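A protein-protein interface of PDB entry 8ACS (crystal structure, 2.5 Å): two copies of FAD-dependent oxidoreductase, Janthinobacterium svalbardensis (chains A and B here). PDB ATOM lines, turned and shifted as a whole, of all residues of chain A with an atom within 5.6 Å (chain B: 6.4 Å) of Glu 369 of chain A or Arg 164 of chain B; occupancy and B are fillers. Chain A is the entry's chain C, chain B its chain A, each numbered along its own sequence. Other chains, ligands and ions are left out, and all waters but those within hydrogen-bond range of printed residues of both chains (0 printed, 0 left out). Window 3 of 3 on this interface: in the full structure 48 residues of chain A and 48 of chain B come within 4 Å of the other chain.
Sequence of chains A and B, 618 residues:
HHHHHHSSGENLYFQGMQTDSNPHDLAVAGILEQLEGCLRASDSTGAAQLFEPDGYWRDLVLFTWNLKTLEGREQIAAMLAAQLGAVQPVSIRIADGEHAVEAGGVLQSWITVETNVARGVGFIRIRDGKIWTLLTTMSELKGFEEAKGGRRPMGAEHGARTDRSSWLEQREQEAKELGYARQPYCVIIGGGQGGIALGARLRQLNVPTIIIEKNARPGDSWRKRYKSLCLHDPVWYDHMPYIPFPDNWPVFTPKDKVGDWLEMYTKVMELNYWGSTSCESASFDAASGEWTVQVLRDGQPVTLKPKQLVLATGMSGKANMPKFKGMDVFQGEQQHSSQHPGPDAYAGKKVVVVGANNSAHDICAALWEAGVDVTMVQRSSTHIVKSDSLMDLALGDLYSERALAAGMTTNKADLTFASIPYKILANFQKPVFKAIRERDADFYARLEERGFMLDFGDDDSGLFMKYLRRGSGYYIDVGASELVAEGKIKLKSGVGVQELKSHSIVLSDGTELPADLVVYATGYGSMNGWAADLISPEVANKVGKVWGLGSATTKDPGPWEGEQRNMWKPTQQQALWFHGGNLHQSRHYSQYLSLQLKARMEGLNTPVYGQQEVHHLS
N of Arg 161 of chain B lies within hydrogen-bond range of OE2 of Glu 369 of chain A (3.1 Å). OE2 of Glu 369 of chain A is in salt-bridge range of NH2 of Arg 164 of chain B. The side-chain amino group (NZ) of Lys 227 of chain A lies within salt-bridge range of the side-chain carboxylate (OE2) of Glu 169 of chain B, 3.1 Å away.
The guanidinium group (NE) of Arg 161 of chain B lies within salt-bridge range of the side-chain carboxylate (OE1) of Glu 157 of chain B (3.1 Å). The backbone carbonyl oxygen (O) of Glu 157 of chain B lies within hydrogen-bond range of the guanidinium group (NH1) of Arg 164 of chain B. The backbone carbonyl oxygen (O) of His 158 of chain B sits at hydrogen-bond distance from the guanidinium group (NH1) of Arg 161 of chain B (3.4 Å). The backbone carbonyl oxygen of Gly 159 of chain B sits at hydrogen-bond distance from the guanidinium group of Arg 161 of chain B, at 3.3 Å. The backbone carbonyl oxygen of Gly 159 of chain B sits at hydrogen-bond distance from the guanidinium group of Arg 164 of chain B, 2.5 Å away. The backbone NH (N) of Ser 166 of chain B sits at hydrogen-bond distance from the side-chain carboxylate (OE1) of Glu 169 of chain B, at 3.0 Å.
Lys 227 of chain A touches Ser 166 of chain B. CB of Ser 228 of chain A touches CD of Arg 164 of chain B, 3.8 Å away. CZ3 of Trp 368 of chain A touches CB of Ala 160 of chain B, 3.6 Å away. Glu 369 of chain A touches Ala 160 of chain B (OE2 to CA, 3.5 Å). O of Glu 369 of chain A touches CG2 of Thr 162 of chain B, 3.3 Å away. Ala 160 of chain B touches Leu 483 of chain A.
No position is printed for both chains. Of the 9 pairs that touch across the chains among the printed residues, none has its exchanged pair printed and touching as well.
Of the printed residues of chain B, Leu 483 of chain A touches Ala 160. Arg 164 of chain B touches two residues of chain A. Of the printed residues of chain A, Ser 166 of chain B touches Lys 227. The nearest residue of chain B that does not touch Glu 369 of chain A is Gly 159 of chain B (4.5 Å). The nearest printed residue of chain A that does not touch Ser 166 of chain B is Ser 228 of chain A (4.7 Å).
Of the 12 printed residues of chain A, 5 touch a printed residue of chain B. Printed residues of chain A that touch a printed residue of chain B: Lys 227, Ser 228, Trp 368, Glu 369 and Leu 483. Hydrophobic or aromatic side chains of chain B within 4 Å of the printed part of chain A: Ala 160. Among the printed residues, 9 pairs touch across the chains.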
ATOM      1  N   TYR A 226     -11.242  -5.265  16.629  1.00  0.00           N
ATOM      2  CA  TYR A 226     -10.663  -4.095  15.999  1.00  0.00           C
ATOM      3  C   TYR A 226     -10.118  -4.410  14.619  1.00  0.00           C
ATOM      4  O   TYR A 226      -9.550  -5.481  14.385  1.00  0.00           O
ATOM      5  CB  TYR A 226      -9.522  -3.524  16.815  1.00  0.00           C
ATOM      6  CG  TYR A 226      -9.003  -2.243  16.173  1.00  0.00           C
ATOM      7  CD1 TYR A 226      -9.838  -1.110  16.058  1.00  0.00           C
ATOM      8  CD2 TYR A 226      -7.687  -2.150  15.686  1.00  0.00           C
ATOM      9  CE1 TYR A 226      -9.375   0.073  15.491  1.00  0.00           C
ATOM     10  CE2 TYR A 226      -7.212  -0.957  15.101  1.00  0.00           C
ATOM     11  CZ  TYR A 226      -8.063   0.154  15.008  1.00  0.00           C
ATOM     12  OH  TYR A 226      -7.599   1.336  14.442  1.00  0.00           O
ATOM     13  N   LYS A 227     -10.167  -3.388  13.753  1.00  0.00           N
ATOM     14  CA  LYS A 227      -9.938  -3.562  12.325  1.00  0.00           C
ATOM     15  C   LYS A 227      -8.748  -4.457  12.028  1.00  0.00           C
ATOM     16  O   LYS A 227      -8.817  -5.335  11.152  1.00  0.00           O
ATOM     17  CB  LYS A 227      -9.703  -2.208  11.649  1.00  0.00           C
ATOM     18  CG  LYS A 227     -10.714  -1.126  11.883  1.00  0.00           C
ATOM     19  CD  LYS A 227     -10.572  -0.121  10.755  1.00  0.00           C
ATOM     20  CE  LYS A 227      -9.131   0.351  10.599  1.00  0.00           C
ATOM     21  NZ  LYS A 227      -9.005   1.487   9.643  1.00  0.00           N
ATOM     22  N   SER A 228      -7.644  -4.231  12.738  1.00  0.00           N
ATOM     23  CA  SER A 228      -6.364  -4.810  12.360  1.00  0.00           C
ATOM     24  C   SER A 228      -6.094  -6.166  13.006  1.00  0.00           C
ATOM     25  O   SER A 228      -5.059  -6.768  12.714  1.00  0.00           O
ATOM     26  CB  SER A 228      -5.235  -3.818  12.677  1.00  0.00           C
ATOM     27  OG  SER A 228      -5.270  -3.445  14.039  1.00  0.00           O
ATOM     28  N   CYS A 364      -3.496   0.469  22.930  1.00  0.00           N
ATOM     29  CA  CYS A 364      -2.488   1.527  22.861  1.00  0.00           C
ATOM     30  C   CYS A 364      -1.825   1.585  21.494  1.00  0.00           C
ATOM     31  O   CYS A 364      -1.539   2.678  20.995  1.00  0.00           O
ATOM     32  CB  CYS A 364      -1.429   1.347  23.946  1.00  0.00           C
ATOM     33  SG  CYS A 364      -2.089   1.682  25.567  1.00  0.00           S
ATOM     34  N   ALA A 365      -1.543   0.420  20.890  1.00  0.00           N
ATOM     35  CA  ALA A 365      -0.913   0.409  19.573  1.00  0.00           C
ATOM     36  C   ALA A 365      -1.848   0.988  18.517  1.00  0.00           C
ATOM     37  O   ALA A 365      -1.397   1.684  17.602  1.00  0.00           O
ATOM     38  CB  ALA A 365      -0.485  -1.013  19.180  1.00  0.00           C
ATOM     39  N   ALA A 366      -3.150   0.726  18.627  1.00  0.00           N
ATOM     40  CA  ALA A 366      -4.082   1.323  17.682  1.00  0.00           C
ATOM     41  C   ALA A 366      -4.187   2.844  17.871  1.00  0.00           C
ATOM     42  O   ALA A 366      -4.214   3.593  16.889  1.00  0.00           O
ATOM     43  CB  ALA A 366      -5.442   0.638  17.805  1.00  0.00           C
ATOM     44  N   LEU A 367      -4.209   3.329  19.121  1.00  0.00           N
ATOM     45  CA  LEU A 367      -4.294   4.773  19.336  1.00  0.00           C
ATOM     46  C   LEU A 367      -3.068   5.498  18.779  1.00  0.00           C
ATOM     47  O   LEU A 367      -3.186   6.611  18.256  1.00  0.00           O
ATOM     48  CB  LEU A 367      -4.495   5.084  20.822  1.00  0.00           C
ATOM     49  CG  LEU A 367      -5.891   4.940  21.454  1.00  0.00           C
ATOM     50  CD1 LEU A 367      -5.794   4.686  22.966  1.00  0.00           C
ATOM     51  CD2 LEU A 367      -6.794   6.146  21.181  1.00  0.00           C
ATOM     52  N   TRP A 368      -1.882   4.891  18.885  1.00  0.00           N
ATOM     53  CA  TRP A 368      -0.679   5.538  18.358  1.00  0.00           C
ATOM     54  C   TRP A 368      -0.624   5.501  16.836  1.00  0.00           C
ATOM     55  O   TRP A 368      -0.118   6.440  16.211  1.00  0.00           O
ATOM     56  CB  TRP A 368       0.578   4.889  18.920  1.00  0.00           C
ATOM     57  CG  TRP A 368       1.858   5.450  18.343  1.00  0.00           C
ATOM     58  CD1 TRP A 368       2.593   6.497  18.823  1.00  0.00           C
ATOM     59  CD2 TRP A 368       2.545   4.984  17.172  1.00  0.00           C
ATOM     60  NE1 TRP A 368       3.701   6.702  18.030  1.00  0.00           N
ATOM     61  CE2 TRP A 368       3.691   5.784  17.011  1.00  0.00           C
ATOM     62  CE3 TRP A 368       2.299   3.969  16.244  1.00  0.00           C
ATOM     63  CZ2 TRP A 368       4.587   5.595  15.969  1.00  0.00           C
ATOM     64  CZ3 TRP A 368       3.180   3.789  15.211  1.00  0.00           C
ATOM     65  CH2 TRP A 368       4.314   4.594  15.082  1.00  0.00           C
ATOM     66  N   GLU A 369      -1.056   4.394  16.230  1.00  0.00           N
ATOM     67  CA  GLU A 369      -1.087   4.306  14.772  1.00  0.00           C
ATOM     68  C   GLU A 369      -2.015   5.358  14.184  1.00  0.00           C
ATOM     69  O   GLU A 369      -1.789   5.833  13.068  1.00  0.00           O
ATOM     70  CB  GLU A 369      -1.495   2.897  14.337  1.00  0.00           C
ATOM     71  CG  GLU A 369      -0.415   1.885  14.643  1.00  0.00           C
ATOM     72  CD  GLU A 369      -0.773   0.452  14.291  1.00  0.00           C
ATOM     73  OE1 GLU A 369      -1.961   0.058  14.395  1.00  0.00           O
ATOM     74  OE2 GLU A 369       0.164  -0.274  13.892  1.00  0.00           O
ATOM     75  N   ALA A 370      -3.071   5.704  14.920  1.00  0.00           N
ATOM     76  CA  ALA A 370      -4.002   6.768  14.600  1.00  0.00           C
ATOM     77  C   ALA A 370      -3.512   8.140  15.043  1.00  0.00           C
ATOM     78  O   ALA A 370      -4.243   9.122  14.885  1.00  0.00           O
ATOM     79  CB  ALA A 370      -5.342   6.467  15.274  1.00  0.00           C
ATOM     80  N   GLY A 371      -2.297   8.249  15.568  1.00  0.00           N
ATOM     81  CA  GLY A 371      -1.802   9.534  16.062  1.00  0.00           C
ATOM     82  C   GLY A 371      -2.577  10.168  17.206  1.00  0.00           C
ATOM     83  O   GLY A 371      -2.743  11.394  17.226  1.00  0.00           O
ATOM     84  N   LEU A 483       6.802  -0.150  20.333  1.00  0.00           N
ATOM     85  CA  LEU A 483       6.310   1.199  20.572  1.00  0.00           C
ATOM     86  C   LEU A 483       6.497   1.605  22.032  1.00  0.00           C
ATOM     87  O   LEU A 483       6.692   2.795  22.324  1.00  0.00           O
ATOM     88  CB  LEU A 483       4.841   1.288  20.176  1.00  0.00           C
ATOM     89  CG  LEU A 483       4.464   1.039  18.725  1.00  0.00           C
ATOM     90  CD1 LEU A 483       2.966   1.080  18.646  1.00  0.00           C
ATOM     91  CD2 LEU A 483       5.082   2.072  17.798  1.00  0.00           C
ATOM     92  N   ALA B 156      -0.714 -11.431   8.513  1.00  0.00           N
ATOM     93  CA  ALA B 156      -0.607 -10.263   9.371  1.00  0.00           C
ATOM     94  C   ALA B 156       0.707  -9.548   9.091  1.00  0.00           C
ATOM     95  O   ALA B 156       1.741 -10.190   8.899  1.00  0.00           O
ATOM     96  CB  ALA B 156      -0.657 -10.662  10.848  1.00  0.00           C
ATOM     97  N   GLU B 157       0.666  -8.221   9.047  1.00  0.00           N
ATOM     98  CA  GLU B 157       1.881  -7.416   8.919  1.00  0.00           C
ATOM     99  C   GLU B 157       2.273  -6.917  10.311  1.00  0.00           C
ATOM    100  O   GLU B 157       1.739  -5.917  10.805  1.00  0.00           O
ATOM    101  CB  GLU B 157       1.684  -6.277   7.925  1.00  0.00           C
ATOM    102  CG  GLU B 157       1.626  -6.757   6.485  1.00  0.00           C
ATOM    103  CD  GLU B 157       1.391  -5.614   5.526  1.00  0.00           C
ATOM    104  OE1 GLU B 157       1.608  -4.456   5.956  1.00  0.00           O
ATOM    105  OE2 GLU B 157       0.989  -5.858   4.360  1.00  0.00           O
ATOM    106  N   HIS B 158       3.210  -7.632  10.941  1.00  0.00           N
ATOM    107  CA  HIS B 158       3.691  -7.281  12.272  1.00  0.00           C
ATOM    108  C   HIS B 158       4.612  -6.060  12.212  1.00  0.00           C
ATOM    109  O   HIS B 158       5.312  -5.828  11.221  1.00  0.00           O
ATOM    110  CB  HIS B 158       4.426  -8.468  12.908  1.00  0.00           C
ATOM    111  CG  HIS B 158       3.545  -9.644  13.220  1.00  0.00           C
ATOM    112  ND1 HIS B 158       4.047 -10.859  13.642  1.00  0.00           N
ATOM    113  CD2 HIS B 158       2.199  -9.792  13.178  1.00  0.00           C
ATOM    114  CE1 HIS B 158       3.049 -11.701  13.850  1.00  0.00           C
ATOM    115  NE2 HIS B 158       1.917 -11.080  13.571  1.00  0.00           N
ATOM    116  N   GLY B 159       4.598  -5.277  13.292  1.00  0.00           N
ATOM    117  CA  GLY B 159       5.308  -4.012  13.360  1.00  0.00           C
ATOM    118  C   GLY B 159       4.374  -2.838  13.146  1.00  0.00           C
ATOM    119  O   GLY B 159       3.508  -2.886  12.266  1.00  0.00           O
ATOM    120  N   ALA B 160       4.540  -1.772  13.923  1.00  0.00           N
ATOM    121  CA  ALA B 160       3.599  -0.660  13.859  1.00  0.00           C
ATOM    122  C   ALA B 160       3.721   0.126  12.549  1.00  0.00           C
ATOM    123  O   ALA B 160       4.810   0.279  11.979  1.00  0.00           O
ATOM    124  CB  ALA B 160       3.799   0.274  15.051  1.00  0.00           C
ATOM    125  N   ARG B 161       2.572   0.627  12.083  1.00  0.00           N
ATOM    126  CA  ARG B 161       2.446   1.420  10.867  1.00  0.00           C
ATOM    127  C   ARG B 161       1.354   2.453  11.091  1.00  0.00           C
ATOM    128  O   ARG B 161       0.465   2.262  11.918  1.00  0.00           O
ATOM    129  CB  ARG B 161       2.062   0.565   9.643  1.00  0.00           C
ATOM    130  CG  ARG B 161       3.082  -0.450   9.168  1.00  0.00           C
ATOM    131  CD  ARG B 161       2.385  -1.657   8.530  1.00  0.00           C
ATOM    132  NE  ARG B 161       3.239  -2.381   7.590  1.00  0.00           N
ATOM    133  CZ  ARG B 161       4.309  -3.090   7.931  1.00  0.00           C
ATOM    134  NH1 ARG B 161       4.721  -3.164   9.192  1.00  0.00           N
ATOM    135  NH2 ARG B 161       4.990  -3.735   6.982  1.00  0.00           N
ATOM    136  N   THR B 162       1.391   3.538  10.318  1.00  0.00           N
ATOM    137  CA  THR B 162       0.239   4.430  10.291  1.00  0.00           C
ATOM    138  C   THR B 162      -0.583   4.296   9.013  1.00  0.00           C
ATOM    139  O   THR B 162      -1.753   4.690   9.006  1.00  0.00           O
ATOM    140  CB  THR B 162       0.674   5.895  10.487  1.00  0.00           C
ATOM    141  OG1 THR B 162       1.640   6.261   9.494  1.00  0.00           O
ATOM    142  CG2 THR B 162       1.267   6.109  11.889  1.00  0.00           C
ATOM    143  N   ASP B 163      -0.011   3.718   7.955  1.00  0.00           N
ATOM    144  CA  ASP B 163      -0.671   3.506   6.660  1.00  0.00           C
ATOM    145  C   ASP B 163      -1.336   2.133   6.563  1.00  0.00           C
ATOM    146  O   ASP B 163      -1.355   1.510   5.489  1.00  0.00           O
ATOM    147  CB  ASP B 163       0.343   3.702   5.532  1.00  0.00           C
ATOM    148  CG  ASP B 163       1.667   2.929   5.762  1.00  0.00           C
ATOM    149  OD1 ASP B 163       1.770   2.142   6.738  1.00  0.00           O
ATOM    150  OD2 ASP B 163       2.612   3.119   4.954  1.00  0.00           O
ATOM    151  N   ARG B 164      -1.912   1.650   7.665  1.00  0.00           N
ATOM    152  CA  ARG B 164      -2.342   0.261   7.761  1.00  0.00           C
ATOM    153  C   ARG B 164      -3.669   0.035   7.037  1.00  0.00           C
ATOM    154  O   ARG B 164      -4.691   0.658   7.356  1.00  0.00           O
ATOM    155  CB  ARG B 164      -2.452  -0.150   9.226  1.00  0.00           C
ATOM    156  CG  ARG B 164      -2.528  -1.653   9.432  1.00  0.00           C
ATOM    157  CD  ARG B 164      -2.415  -2.038  10.892  1.00  0.00           C
ATOM    158  NE  ARG B 164      -1.062  -1.854  11.405  1.00  0.00           N
ATOM    159  CZ  ARG B 164      -0.141  -2.808  11.466  1.00  0.00           C
ATOM    160  NH1 ARG B 164      -0.389  -4.041  11.047  1.00  0.00           N
ATOM    161  NH2 ARG B 164       1.062  -2.516  11.955  1.00  0.00           N
ATOM    162  N   SER B 165      -3.660  -0.885   6.083  1.00  0.00           N
ATOM    163  CA  SER B 165      -4.863  -1.302   5.381  1.00  0.00           C
ATOM    164  C   SER B 165      -5.145  -2.756   5.743  1.00  0.00           C
ATOM    165  O   SER B 165      -4.294  -3.627   5.532  1.00  0.00           O
ATOM    166  CB  SER B 165      -4.709  -1.129   3.868  1.00  0.00           C
ATOM    167  OG  SER B 165      -5.917  -1.420   3.195  1.00  0.00           O
ATOM    168  N   SER B 166      -6.317  -3.007   6.321  1.00  0.00           N
ATOM    169  CA  SER B 166      -6.658  -4.330   6.813  1.00  0.00           C
ATOM    170  C   SER B 166      -7.112  -5.241   5.671  1.00  0.00           C
ATOM    171  O   SER B 166      -7.430  -4.801   4.563  1.00  0.00           O
ATOM    172  CB  SER B 166      -7.754  -4.238   7.865  1.00  0.00           C
ATOM    173  OG  SER B 166      -8.988  -3.931   7.245  1.00  0.00           O
ATOM    174  N   GLU B 169     -10.496  -4.339   4.324  1.00  0.00           N
ATOM    175  CA  GLU B 169     -10.440  -3.139   3.499  1.00  0.00           C
ATOM    176  C   GLU B 169      -9.899  -3.431   2.104  1.00  0.00           C
ATOM    177  O   GLU B 169     -10.444  -2.945   1.105  1.00  0.00           O
ATOM    178  CB  GLU B 169      -9.601  -2.072   4.196  1.00  0.00           C
ATOM    179  CG  GLU B 169     -10.330  -1.454   5.368  1.00  0.00           C
ATOM    180  CD  GLU B 169      -9.453  -0.541   6.191  1.00  0.00           C
ATOM    181  OE1 GLU B 169      -8.210  -0.631   6.052  1.00  0.00           O
ATOM    182  OE2 GLU B 169     -10.018   0.251   6.982  1.00  0.00           O
